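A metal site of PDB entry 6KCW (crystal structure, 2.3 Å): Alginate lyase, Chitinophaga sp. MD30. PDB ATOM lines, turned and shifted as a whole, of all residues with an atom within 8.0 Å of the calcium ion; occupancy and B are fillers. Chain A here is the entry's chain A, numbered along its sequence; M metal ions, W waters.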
ATOM      1  N   ILE A   8      -7.551 -34.669  15.476  1.00  0.00           N
ATOM      2  CA  ILE A   8      -7.105 -33.343  15.858  1.00  0.00           C
ATOM      3  C   ILE A   8      -7.662 -33.091  17.256  1.00  0.00           C
ATOM      4  O   ILE A   8      -8.873 -32.997  17.442  1.00  0.00           O
ATOM      5  CB  ILE A   8      -7.597 -32.248  14.876  1.00  0.00           C
ATOM      6  CG1 ILE A   8      -7.388 -32.693  13.420  1.00  0.00           C
ATOM      7  CG2 ILE A   8      -6.866 -30.942  15.127  1.00  0.00           C
ATOM      8  CD1 ILE A   8      -8.077 -31.816  12.371  1.00  0.00           C
ATOM      9  N   ASN A   9      -6.769 -32.997  18.244  1.00  0.00           N
ATOM     10  CA  ASN A   9      -7.177 -32.655  19.595  1.00  0.00           C
ATOM     11  C   ASN A   9      -6.566 -31.350  20.064  1.00  0.00           C
ATOM     12  O   ASN A   9      -6.765 -30.963  21.214  1.00  0.00           O
ATOM     13  CB  ASN A   9      -6.813 -33.766  20.582  1.00  0.00           C
ATOM     14  CG  ASN A   9      -5.345 -34.132  20.521  1.00  0.00           C
ATOM     15  OD1 ASN A   9      -4.522 -33.409  19.951  1.00  0.00           O
ATOM     16  ND2 ASN A   9      -5.007 -35.284  21.093  1.00  0.00           N
ATOM     17  N   TRP A  10      -5.803 -30.672  19.205  1.00  0.00           N
ATOM     18  CA  TRP A  10      -5.315 -29.323  19.473  1.00  0.00           C
ATOM     19  C   TRP A  10      -4.457 -29.261  20.740  1.00  0.00           C
ATOM     20  O   TRP A  10      -4.320 -28.191  21.340  1.00  0.00           O
ATOM     21  CB  TRP A  10      -6.483 -28.339  19.545  1.00  0.00           C
ATOM     22  CG  TRP A  10      -7.231 -28.246  18.251  1.00  0.00           C
ATOM     23  CD1 TRP A  10      -6.855 -27.540  17.145  1.00  0.00           C
ATOM     24  CD2 TRP A  10      -8.470 -28.888  17.916  1.00  0.00           C
ATOM     25  NE1 TRP A  10      -7.779 -27.696  16.142  1.00  0.00           N
ATOM     26  CE2 TRP A  10      -8.787 -28.515  16.588  1.00  0.00           C
ATOM     27  CE3 TRP A  10      -9.347 -29.730  18.603  1.00  0.00           C
ATOM     28  CZ2 TRP A  10      -9.931 -28.965  15.929  1.00  0.00           C
ATOM     29  CZ3 TRP A  10     -10.490 -30.181  17.944  1.00  0.00           C
ATOM     30  CH2 TRP A  10     -10.767 -29.791  16.631  1.00  0.00           C
ATOM     31  N   ASN A  11      -3.899 -30.390  21.161  1.00  0.00           N
ATOM     32  CA  ASN A  11      -3.111 -30.430  22.381  1.00  0.00           C
ATOM     33  C   ASN A  11      -1.667 -29.990  22.184  1.00  0.00           C
ATOM     34  O   ASN A  11      -1.000 -29.622  23.145  1.00  0.00           O
ATOM     35  CB  ASN A  11      -3.161 -31.830  22.983  1.00  0.00           C
ATOM     36  CG  ASN A  11      -4.478 -32.118  23.611  1.00  0.00           C
ATOM     37  OD1 ASN A  11      -5.337 -31.243  23.669  1.00  0.00           O
ATOM     38  ND2 ASN A  11      -4.663 -33.344  24.098  1.00  0.00           N
ATOM     39  N   ASN A  12      -1.185 -30.043  20.943  1.00  0.00           N
ATOM     40  CA  ASN A  12       0.115 -29.497  20.568  1.00  0.00           C
ATOM     41  C   ASN A  12       0.068 -27.990  20.342  1.00  0.00           C
ATOM     42  O   ASN A  12       1.091 -27.420  19.963  1.00  0.00           O
ATOM     43  CB  ASN A  12       0.606 -30.185  19.303  1.00  0.00           C
ATOM     44  CG  ASN A  12      -0.372 -30.035  18.131  1.00  0.00           C
ATOM     45  OD1 ASN A  12      -1.586 -30.164  18.285  1.00  0.00           O
ATOM     46  ND2 ASN A  12       0.174 -29.754  16.955  1.00  0.00           N
ATOM     47  N   TYR A  13      -1.073 -27.345  20.546  1.00  0.00           N
ATOM     48  CA  TYR A  13      -1.200 -25.918  20.269  1.00  0.00           C
ATOM     49  C   TYR A  13      -1.076 -25.116  21.542  1.00  0.00           C
ATOM     50  O   TYR A  13      -1.499 -25.548  22.625  1.00  0.00           O
ATOM     51  CB  TYR A  13      -2.525 -25.574  19.591  1.00  0.00           C
ATOM     52  CG  TYR A  13      -2.453 -25.802  18.115  1.00  0.00           C
ATOM     53  CD1 TYR A  13      -1.876 -24.857  17.282  1.00  0.00           C
ATOM     54  CD2 TYR A  13      -2.926 -26.985  17.560  1.00  0.00           C
ATOM     55  CE1 TYR A  13      -1.779 -25.069  15.920  1.00  0.00           C
ATOM     56  CE2 TYR A  13      -2.839 -27.221  16.214  1.00  0.00           C
ATOM     57  CZ  TYR A  13      -2.267 -26.248  15.393  1.00  0.00           C
ATOM     58  OH  TYR A  13      -2.180 -26.497  14.052  1.00  0.00           O
ATOM     59  N   ILE A  40      -7.226 -21.162  20.125  1.00  0.00           N
ATOM     60  CA  ILE A  40      -6.970 -22.303  21.001  1.00  0.00           C
ATOM     61  C   ILE A  40      -7.035 -21.810  22.437  1.00  0.00           C
ATOM     62  O   ILE A  40      -6.230 -20.969  22.861  1.00  0.00           O
ATOM     63  CB  ILE A  40      -5.610 -22.963  20.703  1.00  0.00           C
ATOM     64  CG1 ILE A  40      -5.537 -23.435  19.264  1.00  0.00           C
ATOM     65  CG2 ILE A  40      -5.431 -24.204  21.596  1.00  0.00           C
ATOM     66  CD1 ILE A  40      -6.469 -24.628  18.982  1.00  0.00           C
ATOM     67  N   SER A  41      -7.999 -22.328  23.186  1.00  0.00           N
ATOM     68  CA  SER A  41      -8.170 -21.993  24.598  1.00  0.00           C
ATOM     69  C   SER A  41      -7.948 -23.281  25.394  1.00  0.00           C
ATOM     70  O   SER A  41      -8.827 -24.152  25.455  1.00  0.00           O
ATOM     71  CB  SER A  41      -9.555 -21.399  24.831  1.00  0.00           C
ATOM     72  OG  SER A  41      -9.824 -21.225  26.210  1.00  0.00           O
ATOM     73  N   ASP A  42      -6.754 -23.409  25.987  1.00  0.00           N
ATOM     74  CA  ASP A  42      -6.423 -24.536  26.881  1.00  0.00           C
ATOM     75  C   ASP A  42      -6.576 -25.877  26.174  1.00  0.00           C
ATOM     76  O   ASP A  42      -7.234 -26.801  26.670  1.00  0.00           O
ATOM     77  CB  ASP A  42      -7.275 -24.499  28.150  1.00  0.00           C
ATOM     78  CG  ASP A  42      -6.474 -24.151  29.383  1.00  0.00           C
ATOM     79  OD1 ASP A  42      -5.343 -23.611  29.241  1.00  0.00           O
ATOM     80  OD2 ASP A  42      -6.961 -24.413  30.503  1.00  0.00           O
ATOM     81  N   GLY A  43      -5.949 -26.012  25.014  1.00  0.00           N
ATOM     82  CA  GLY A  43      -5.952 -27.276  24.309  1.00  0.00           C
ATOM     83  C   GLY A  43      -7.227 -27.616  23.568  1.00  0.00           C
ATOM     84  O   GLY A  43      -7.317 -28.707  23.006  1.00  0.00           O
ATOM     85  N   THR A  44      -8.214 -26.718  23.529  1.00  0.00           N
ATOM     86  CA  THR A  44      -9.421 -26.899  22.722  1.00  0.00           C
ATOM     87  C   THR A  44      -9.538 -25.770  21.722  1.00  0.00           C
ATOM     88  O   THR A  44      -8.864 -24.741  21.817  1.00  0.00           O
ATOM     89  CB  THR A  44     -10.691 -26.949  23.584  1.00  0.00           C
ATOM     90  OG1 THR A  44     -11.095 -25.611  23.932  1.00  0.00           O
ATOM     91  CG2 THR A  44     -10.450 -27.742  24.858  1.00  0.00           C
ATOM     92  N   LEU A  45     -10.428 -25.952  20.762  1.00  0.00           N
ATOM     93  CA  LEU A  45     -10.694 -24.946  19.738  1.00  0.00           C
ATOM     94  C   LEU A  45     -11.916 -24.134  20.136  1.00  0.00           C
ATOM     95  O   LEU A  45     -13.037 -24.671  20.185  1.00  0.00           O
ATOM     96  CB  LEU A  45     -10.882 -25.595  18.370  1.00  0.00           C
ATOM     97  CG  LEU A  45     -11.363 -24.745  17.194  1.00  0.00           C
ATOM     98  CD1 LEU A  45     -10.587 -23.427  17.070  1.00  0.00           C
ATOM     99  CD2 LEU A  45     -11.244 -25.568  15.923  1.00  0.00           C
ATOM    100  N   ASP A  77     -15.896 -33.499  20.775  1.00  0.00           N
ATOM    101  CA  ASP A  77     -16.516 -32.965  21.977  1.00  0.00           C
ATOM    102  C   ASP A  77     -16.855 -31.512  21.739  1.00  0.00           C
ATOM    103  O   ASP A  77     -16.182 -30.814  20.974  1.00  0.00           O
ATOM    104  CB  ASP A  77     -15.600 -33.092  23.197  1.00  0.00           C
ATOM    105  CG  ASP A  77     -15.367 -34.524  23.571  1.00  0.00           C
ATOM    106  OD1 ASP A  77     -16.356 -35.294  23.573  1.00  0.00           O
ATOM    107  OD2 ASP A  77     -14.194 -34.889  23.839  1.00  0.00           O
ATOM    108  N   TYR A 232     -14.650 -26.813  20.911  1.00  0.00           N
ATOM    109  CA  TYR A 232     -14.576 -28.154  20.367  1.00  0.00           C
ATOM    110  C   TYR A 232     -13.249 -28.809  20.746  1.00  0.00           C
ATOM    111  O   TYR A 232     -12.245 -28.134  21.010  1.00  0.00           O
ATOM    112  CB  TYR A 232     -14.735 -28.137  18.844  1.00  0.00           C
ATOM    113  CG  TYR A 232     -15.972 -27.397  18.367  1.00  0.00           C
ATOM    114  CD1 TYR A 232     -17.230 -27.996  18.420  1.00  0.00           C
ATOM    115  CD2 TYR A 232     -15.891 -26.099  17.867  1.00  0.00           C
ATOM    116  CE1 TYR A 232     -18.369 -27.327  17.978  1.00  0.00           C
ATOM    117  CE2 TYR A 232     -17.015 -25.434  17.440  1.00  0.00           C
ATOM    118  CZ  TYR A 232     -18.257 -26.046  17.499  1.00  0.00           C
ATOM    119  OH  TYR A 232     -19.382 -25.395  17.078  1.00  0.00           O
ATOM    120  N   ASP A 233     -13.240 -30.149  20.736  1.00  0.00           N
ATOM    121  CA  ASP A 233     -12.035 -30.902  21.062  1.00  0.00           C
ATOM    122  C   ASP A 233     -12.147 -32.311  20.493  1.00  0.00           C
ATOM    123  O   ASP A 233     -13.249 -32.826  20.253  1.00  0.00           O
ATOM    124  CB  ASP A 233     -11.820 -30.962  22.585  1.00  0.00           C
ATOM    125  CG  ASP A 233     -10.368 -31.156  22.956  1.00  0.00           C
ATOM    126  OD1 ASP A 233      -9.580 -31.554  22.071  1.00  0.00           O
ATOM    127  OD2 ASP A 233     -10.026 -30.914  24.134  1.00  0.00           O
ATOM    128  N   ASN A 234     -10.978 -32.920  20.270  1.00  0.00           N
ATOM    129  CA  ASN A 234     -10.867 -34.363  20.059  1.00  0.00           C
ATOM    130  C   ASN A 234     -11.623 -34.837  18.825  1.00  0.00           C
ATOM    131  O   ASN A 234     -12.372 -35.817  18.867  1.00  0.00           O
ATOM    132  CB  ASN A 234     -11.347 -35.116  21.304  1.00  0.00           C
ATOM    133  CG  ASN A 234     -10.501 -34.814  22.526  1.00  0.00           C
ATOM    134  OD1 ASN A 234      -9.276 -34.848  22.468  1.00  0.00           O
ATOM    135  ND2 ASN A 234     -11.147 -34.483  23.639  1.00  0.00           N
ATOM    136  N   LEU A 235     -11.397 -34.151  17.706  1.00  0.00           N
ATOM    137  CA  LEU A 235     -12.068 -34.480  16.455  1.00  0.00           C
ATOM    138  C   LEU A 235     -11.426 -35.710  15.820  1.00  0.00           C
ATOM    139  O   LEU A 235     -10.232 -35.694  15.514  1.00  0.00           O
ATOM    140  CB  LEU A 235     -12.017 -33.309  15.488  1.00  0.00           C
ATOM    141  CG  LEU A 235     -12.540 -33.662  14.084  1.00  0.00           C
ATOM    142  CD1 LEU A 235     -14.051 -33.939  14.107  1.00  0.00           C
ATOM    143  CD2 LEU A 235     -12.195 -32.606  13.079  1.00  0.00           C
HETATM  144 CA    CA M   1      -7.500 -30.998  23.300  1.00  0.00          CA
HETATM  145  O   HOH W   1      -6.865 -30.926  25.340  1.00  0.00           O
HETATM  146  O   HOH W   2      -7.607 -33.643  23.678  1.00  0.00           O
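The side-chain carboxylate of Asp 233 sits close to the side-chain amide oxygen of Asn 234 (3.3 Å). O of Asp 233 sits at hydrogen-bond distance from N of Asp 77 (2.8 Å).
Of the 17 residues printed, 4 come within 4 Å of the calcium ion. The nearest printed residue that does not touch the calcium ion is Asn 234 (4.3 Å).
Water W1 is bound to the calcium ion (2.1 Å). OD1 of Asn 11 binds the calcium ion, 2.2 Å away. O of Asn 9 binds the calcium ion (2.2 Å). O of Gly 43 binds the calcium ion, 2.3 Å away. OD1 of Asp 233 is bound to the calcium ion. OD2 of Asp 233 is bound to the calcium ion. The calcium ion is bound by water W2.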
